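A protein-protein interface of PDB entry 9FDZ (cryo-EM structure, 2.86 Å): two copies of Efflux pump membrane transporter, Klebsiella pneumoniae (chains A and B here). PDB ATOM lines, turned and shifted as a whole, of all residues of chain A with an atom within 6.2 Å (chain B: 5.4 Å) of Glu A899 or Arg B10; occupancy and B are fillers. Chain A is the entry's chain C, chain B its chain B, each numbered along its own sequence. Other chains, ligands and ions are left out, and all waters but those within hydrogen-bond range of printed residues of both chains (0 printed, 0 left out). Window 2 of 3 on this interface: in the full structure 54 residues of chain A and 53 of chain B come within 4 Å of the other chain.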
ATOM      1  N   LEU A 894      18.684  30.200 -23.250  1.00  0.00           N
ATOM      2  CA  LEU A 894      18.245  29.333 -24.339  1.00  0.00           C
ATOM      3  C   LEU A 894      18.227  27.872 -23.913  1.00  0.00           C
ATOM      4  O   LEU A 894      17.308  27.125 -24.268  1.00  0.00           O
ATOM      5  CB  LEU A 894      19.145  29.526 -25.556  1.00  0.00           C
ATOM      6  CG  LEU A 894      18.948  30.829 -26.331  1.00  0.00           C
ATOM      7  CD1 LEU A 894      20.068  31.026 -27.333  1.00  0.00           C
ATOM      8  CD2 LEU A 894      17.599  30.836 -27.024  1.00  0.00           C
ATOM      9  N   ALA A 895      19.239  27.442 -23.158  1.00  0.00           N
ATOM     10  CA  ALA A 895      19.273  26.063 -22.682  1.00  0.00           C
ATOM     11  C   ALA A 895      18.104  25.771 -21.752  1.00  0.00           C
ATOM     12  O   ALA A 895      17.498  24.697 -21.819  1.00  0.00           O
ATOM     13  CB  ALA A 895      20.601  25.782 -21.982  1.00  0.00           C
ATOM     14  N   ALA A 896      17.777  26.718 -20.872  1.00  0.00           N
ATOM     15  CA  ALA A 896      16.661  26.525 -19.954  1.00  0.00           C
ATOM     16  C   ALA A 896      15.341  26.424 -20.706  1.00  0.00           C
ATOM     17  O   ALA A 896      14.499  25.573 -20.398  1.00  0.00           O
ATOM     18  CB  ALA A 896      16.618  27.670 -18.944  1.00  0.00           C
ATOM     19  N   LEU A 897      15.141  27.289 -21.702  1.00  0.00           N
ATOM     20  CA  LEU A 897      13.860  27.331 -22.397  1.00  0.00           C
ATOM     21  C   LEU A 897      13.682  26.137 -23.325  1.00  0.00           C
ATOM     22  O   LEU A 897      12.580  25.589 -23.434  1.00  0.00           O
ATOM     23  CB  LEU A 897      13.731  28.636 -23.180  1.00  0.00           C
ATOM     24  CG  LEU A 897      13.465  29.899 -22.363  1.00  0.00           C
ATOM     25  CD1 LEU A 897      13.680  31.136 -23.215  1.00  0.00           C
ATOM     26  CD2 LEU A 897      12.059  29.878 -21.792  1.00  0.00           C
ATOM     27  N   TYR A 898      14.749  25.718 -24.003  1.00  0.00           N
ATOM     28  CA  TYR A 898      14.644  24.720 -25.058  1.00  0.00           C
ATOM     29  C   TYR A 898      15.190  23.358 -24.647  1.00  0.00           C
ATOM     30  O   TYR A 898      15.168  22.426 -25.459  1.00  0.00           O
ATOM     31  CB  TYR A 898      15.348  25.229 -26.315  1.00  0.00           C
ATOM     32  CG  TYR A 898      14.577  26.336 -26.999  1.00  0.00           C
ATOM     33  CD1 TYR A 898      13.237  26.555 -26.706  1.00  0.00           C
ATOM     34  CD2 TYR A 898      15.191  27.177 -27.915  1.00  0.00           C
ATOM     35  CE1 TYR A 898      12.528  27.566 -27.316  1.00  0.00           C
ATOM     36  CE2 TYR A 898      14.488  28.193 -28.532  1.00  0.00           C
ATOM     37  CZ  TYR A 898      13.157  28.383 -28.228  1.00  0.00           C
ATOM     38  OH  TYR A 898      12.454  29.394 -28.837  1.00  0.00           O
ATOM     39  N   GLU A 899      15.675  23.222 -23.414  1.00  0.00           N
ATOM     40  CA  GLU A 899      16.039  21.927 -22.836  1.00  0.00           C
ATOM     41  C   GLU A 899      17.084  21.204 -23.685  1.00  0.00           C
ATOM     42  O   GLU A 899      16.877  20.083 -24.153  1.00  0.00           O
ATOM     43  CB  GLU A 899      14.795  21.059 -22.639  1.00  0.00           C
ATOM     44  CG  GLU A 899      14.980  19.878 -21.699  1.00  0.00           C
ATOM     45  CD  GLU A 899      15.307  20.303 -20.285  1.00  0.00           C
ATOM     46  OE1 GLU A 899      14.865  21.397 -19.874  1.00  0.00           O
ATOM     47  OE2 GLU A 899      16.001  19.539 -19.582  1.00  0.00           O
ATOM     48  N   SER A 900      18.221  21.863 -23.890  1.00  0.00           N
ATOM     49  CA  SER A 900      19.317  21.251 -24.628  1.00  0.00           C
ATOM     50  C   SER A 900      20.603  22.005 -24.332  1.00  0.00           C
ATOM     51  O   SER A 900      20.571  23.200 -24.031  1.00  0.00           O
ATOM     52  CB  SER A 900      19.040  21.245 -26.134  1.00  0.00           C
ATOM     53  OG  SER A 900      20.139  20.709 -26.848  1.00  0.00           O
ATOM     54  N   TRP A 901      21.729  21.296 -24.416  1.00  0.00           N
ATOM     55  CA  TRP A 901      23.027  21.940 -24.249  1.00  0.00           C
ATOM     56  C   TRP A 901      23.643  22.332 -25.584  1.00  0.00           C
ATOM     57  O   TRP A 901      24.426  23.285 -25.644  1.00  0.00           O
ATOM     58  CB  TRP A 901      23.986  21.020 -23.492  1.00  0.00           C
ATOM     59  CG  TRP A 901      23.681  20.872 -22.035  1.00  0.00           C
ATOM     60  CD1 TRP A 901      23.404  19.714 -21.372  1.00  0.00           C
ATOM     61  CD2 TRP A 901      23.639  21.915 -21.053  1.00  0.00           C
ATOM     62  NE1 TRP A 901      23.184  19.970 -20.042  1.00  0.00           N
ATOM     63  CE2 TRP A 901      23.323  21.314 -19.820  1.00  0.00           C
ATOM     64  CE3 TRP A 901      23.835  23.298 -21.098  1.00  0.00           C
ATOM     65  CZ2 TRP A 901      23.196  22.047 -18.644  1.00  0.00           C
ATOM     66  CZ3 TRP A 901      23.709  24.023 -19.929  1.00  0.00           C
ATOM     67  CH2 TRP A 901      23.393  23.397 -18.720  1.00  0.00           C
ATOM     68  N   LEU A 903      21.675  22.733 -28.609  1.00  0.00           N
ATOM     69  CA  LEU A 903      20.787  23.612 -29.364  1.00  0.00           C
ATOM     70  C   LEU A 903      21.104  25.092 -29.171  1.00  0.00           C
ATOM     71  O   LEU A 903      21.130  25.819 -30.179  1.00  0.00           O
ATOM     72  CB  LEU A 903      19.329  23.301 -29.004  1.00  0.00           C
ATOM     73  CG  LEU A 903      18.233  23.985 -29.815  1.00  0.00           C
ATOM     74  CD1 LEU A 903      17.068  23.039 -30.038  1.00  0.00           C
ATOM     75  CD2 LEU A 903      17.763  25.244 -29.112  1.00  0.00           C
ATOM     76  N   ARG A 956      13.135  22.355 -34.150  1.00  0.00           N
ATOM     77  CA  ARG A 956      13.036  21.519 -32.958  1.00  0.00           C
ATOM     78  C   ARG A 956      11.645  20.914 -32.822  1.00  0.00           C
ATOM     79  O   ARG A 956      11.501  19.742 -32.455  1.00  0.00           O
ATOM     80  CB  ARG A 956      13.392  22.340 -31.720  1.00  0.00           C
ATOM     81  CG  ARG A 956      13.266  21.591 -30.410  1.00  0.00           C
ATOM     82  CD  ARG A 956      13.415  22.535 -29.233  1.00  0.00           C
ATOM     83  NE  ARG A 956      13.366  21.832 -27.958  1.00  0.00           N
ATOM     84  CZ  ARG A 956      12.306  21.798 -27.163  1.00  0.00           C
ATOM     85  NH1 ARG A 956      11.184  22.422 -27.483  1.00  0.00           N
ATOM     86  NH2 ARG A 956      12.372  21.124 -26.019  1.00  0.00           N
ATOM     87  N   PHE B   6       7.775  19.351 -11.893  1.00  0.00           N
ATOM     88  CA  PHE B   6       8.003  19.985 -13.186  1.00  0.00           C
ATOM     89  C   PHE B   6       9.480  19.980 -13.558  1.00  0.00           C
ATOM     90  O   PHE B   6       9.819  19.983 -14.745  1.00  0.00           O
ATOM     91  CB  PHE B   6       7.449  21.411 -13.159  1.00  0.00           C
ATOM     92  CG  PHE B   6       7.945  22.286 -14.275  1.00  0.00           C
ATOM     93  CD1 PHE B   6       7.340  22.255 -15.518  1.00  0.00           C
ATOM     94  CD2 PHE B   6       8.997  23.163 -14.072  1.00  0.00           C
ATOM     95  CE1 PHE B   6       7.787  23.065 -16.542  1.00  0.00           C
ATOM     96  CE2 PHE B   6       9.448  23.975 -15.093  1.00  0.00           C
ATOM     97  CZ  PHE B   6       8.842  23.925 -16.329  1.00  0.00           C
ATOM     98  N   PHE B   7      10.367  19.959 -12.563  1.00  0.00           N
ATOM     99  CA  PHE B   7      11.801  20.032 -12.803  1.00  0.00           C
ATOM    100  C   PHE B   7      12.461  18.669 -12.951  1.00  0.00           C
ATOM    101  O   PHE B   7      13.596  18.600 -13.435  1.00  0.00           O
ATOM    102  CB  PHE B   7      12.486  20.797 -11.670  1.00  0.00           C
ATOM    103  CG  PHE B   7      12.254  22.276 -11.713  1.00  0.00           C
ATOM    104  CD1 PHE B   7      12.989  23.080 -12.563  1.00  0.00           C
ATOM    105  CD2 PHE B   7      11.297  22.863 -10.906  1.00  0.00           C
ATOM    106  CE1 PHE B   7      12.777  24.441 -12.606  1.00  0.00           C
ATOM    107  CE2 PHE B   7      11.080  24.224 -10.945  1.00  0.00           C
ATOM    108  CZ  PHE B   7      11.822  25.014 -11.795  1.00  0.00           C
ATOM    109  N   ILE B   8      11.793  17.592 -12.540  1.00  0.00           N
ATOM    110  CA  ILE B   8      12.377  16.263 -12.692  1.00  0.00           C
ATOM    111  C   ILE B   8      12.505  15.905 -14.167  1.00  0.00           C
ATOM    112  O   ILE B   8      13.482  15.273 -14.585  1.00  0.00           O
ATOM    113  CB  ILE B   8      11.547  15.222 -11.924  1.00  0.00           C
ATOM    114  CG1 ILE B   8      11.381  15.648 -10.467  1.00  0.00           C
ATOM    115  CG2 ILE B   8      12.201  13.854 -12.002  1.00  0.00           C
ATOM    116  CD1 ILE B   8      10.643  14.642  -9.620  1.00  0.00           C
ATOM    117  N   ASP B   9      11.526  16.305 -14.977  1.00  0.00           N
ATOM    118  CA  ASP B   9      11.552  16.034 -16.407  1.00  0.00           C
ATOM    119  C   ASP B   9      12.434  17.003 -17.182  1.00  0.00           C
ATOM    120  O   ASP B   9      12.660  16.787 -18.377  1.00  0.00           O
ATOM    121  CB  ASP B   9      10.132  16.077 -16.972  1.00  0.00           C
ATOM    122  CG  ASP B   9       9.223  15.047 -16.337  1.00  0.00           C
ATOM    123  OD1 ASP B   9       9.733  14.007 -15.872  1.00  0.00           O
ATOM    124  OD2 ASP B   9       7.997  15.280 -16.300  1.00  0.00           O
ATOM    125  N   ARG B  10      12.933  18.055 -16.539  1.00  0.00           N
ATOM    126  CA  ARG B  10      13.757  19.073 -17.190  1.00  0.00           C
ATOM    127  C   ARG B  10      15.033  19.275 -16.384  1.00  0.00           C
ATOM    128  O   ARG B  10      15.181  20.273 -15.668  1.00  0.00           O
ATOM    129  CB  ARG B  10      12.985  20.385 -17.335  1.00  0.00           C
ATOM    130  CG  ARG B  10      11.732  20.268 -18.180  1.00  0.00           C
ATOM    131  CD  ARG B  10      10.851  21.495 -18.041  1.00  0.00           C
ATOM    132  NE  ARG B  10       9.661  21.410 -18.880  1.00  0.00           N
ATOM    133  CZ  ARG B  10       8.620  20.626 -18.634  1.00  0.00           C
ATOM    134  NH1 ARG B  10       8.578  19.847 -17.565  1.00  0.00           N
ATOM    135  NH2 ARG B  10       7.593  20.630 -19.476  1.00  0.00           N
ATOM    136  N   PRO B  11      15.974  18.332 -16.467  1.00  0.00           N
ATOM    137  CA  PRO B  11      17.228  18.490 -15.713  1.00  0.00           C
ATOM    138  C   PRO B  11      18.019  19.723 -16.110  1.00  0.00           C
ATOM    139  O   PRO B  11      18.655  20.350 -15.254  1.00  0.00           O
ATOM    140  CB  PRO B  11      17.995  17.200 -16.035  1.00  0.00           C
ATOM    141  CG  PRO B  11      16.975  16.251 -16.565  1.00  0.00           C
ATOM    142  CD  PRO B  11      15.960  17.093 -17.259  1.00  0.00           C
ATOM    143  N   ILE B  12      17.999  20.088 -17.393  1.00  0.00           N
ATOM    144  CA  ILE B  12      18.797  21.216 -17.859  1.00  0.00           C
ATOM    145  C   ILE B  12      18.229  22.529 -17.339  1.00  0.00           C
ATOM    146  O   ILE B  12      18.978  23.443 -16.973  1.00  0.00           O
ATOM    147  CB  ILE B  12      18.897  21.194 -19.393  1.00  0.00           C
ATOM    148  CG1 ILE B  12      19.613  19.923 -19.846  1.00  0.00           C
ATOM    149  CG2 ILE B  12      19.633  22.417 -19.899  1.00  0.00           C
ATOM    150  CD1 ILE B  12      19.629  19.725 -21.335  1.00  0.00           C
ATOM    151  N   PHE B  13      16.901  22.652 -17.300  1.00  0.00           N
ATOM    152  CA  PHE B  13      16.292  23.837 -16.705  1.00  0.00           C
ATOM    153  C   PHE B  13      16.649  23.949 -15.230  1.00  0.00           C
ATOM    154  O   PHE B  13      16.967  25.039 -14.740  1.00  0.00           O
ATOM    155  CB  PHE B  13      14.775  23.795 -16.894  1.00  0.00           C
ATOM    156  CG  PHE B  13      14.069  25.059 -16.484  1.00  0.00           C
ATOM    157  CD1 PHE B  13      14.751  26.258 -16.385  1.00  0.00           C
ATOM    158  CD2 PHE B  13      12.717  25.045 -16.196  1.00  0.00           C
ATOM    159  CE1 PHE B  13      14.100  27.413 -16.006  1.00  0.00           C
ATOM    160  CE2 PHE B  13      12.063  26.198 -15.817  1.00  0.00           C
ATOM    161  CZ  PHE B  13      12.756  27.383 -15.723  1.00  0.00           C
ATOM    162  N   ALA B  14      16.604  22.831 -14.503  1.00  0.00           N
ATOM    163  CA  ALA B  14      17.003  22.847 -13.100  1.00  0.00           C
ATOM    164  C   ALA B  14      18.480  23.185 -12.950  1.00  0.00           C
ATOM    165  O   ALA B  14      18.860  23.964 -12.069  1.00  0.00           O
ATOM    166  CB  ALA B  14      16.691  21.500 -12.453  1.00  0.00           C
ATOM    167  N   ALA B  15      19.328  22.608 -13.803  1.00  0.00           N
ATOM    168  CA  ALA B  15      20.761  22.876 -13.725  1.00  0.00           C
ATOM    169  C   ALA B  15      21.074  24.332 -14.048  1.00  0.00           C
ATOM    170  O   ALA B  15      21.917  24.952 -13.392  1.00  0.00           O
ATOM    171  CB  ALA B  15      21.522  21.945 -14.665  1.00  0.00           C
ATOM    172  N   ALA B 493      16.071  16.028  -9.999  1.00  0.00           N
ATOM    173  CA  ALA B 493      16.485  15.810 -11.380  1.00  0.00           C
ATOM    174  C   ALA B 493      17.778  15.012 -11.448  1.00  0.00           C
ATOM    175  O   ALA B 493      17.911  14.101 -12.272  1.00  0.00           O
ATOM    176  CB  ALA B 493      16.642  17.150 -12.097  1.00  0.00           C
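Arg B10 touches one residue of chain A. Of the printed residues of chain B, Trp A901 touches Ile B12. Printed residues of chain A within 4 Å of Pro B11: Glu A899 (3.3 Å). Of the printed residues of chain A, Ile B12 touches Ala A895, Glu A899, Ser A900 and Trp A901. Of the printed residues of chain A, Phe B13 touches Ala A896 (3.5 Å) and Glu A899 (3.5 Å). Printed residues of chain B within 4 Å of Ala A896: Phe B13 (3.5 Å). Leu A897 touches none of the printed residues of chain B. Asp B9 touches none of the printed residues of chain A. The nearest residue of chain B that does not touch Glu A899 is Asp B9 (4.5 Å). The nearest residue of chain A that does not touch Arg B10 is Ala A896 (6.0 Å).
No position is printed for both chains. Of the 8 pairs that touch across the chains among the printed residues, none has its exchanged pair printed and touching as well.
OE2 of Glu A899 is in hydrogen-bond range of N of Ile B12 (3.0 Å). The side-chain carboxylate (OE2) of Glu A899 sits close to the backbone nitrogen (N) of Pro B11.
O of Phe B6 lies within hydrogen-bond range of NH1 of Arg B10, 3.1 Å away. OG of Ser A900 lies within hydrogen-bond range of N of Leu A903.
Hydrophobic or aromatic side chains of chain B that line the printed part of chain A: Pro B11, Ile B12 and Phe B13. Of the 10 printed residues of chain A, 5 touch a printed residue of chain B. Among the printed residues, 8 pairs touch across the chains.
Ile B12 touches Ala A895 (CG2 to O, 3.7 Å). CB of Ala A896 touches CD1 of Phe B13, at 3.5 Å. CA of Arg B10 touches OE2 of Glu A899 (3.3 Å). Glu A899 touches Phe B13. N of Ser A900 touches CD1 of Ile B12 (3.6 Å). Ile B12 touches Trp A901 (CG1 to NE1, 3.6 Å).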
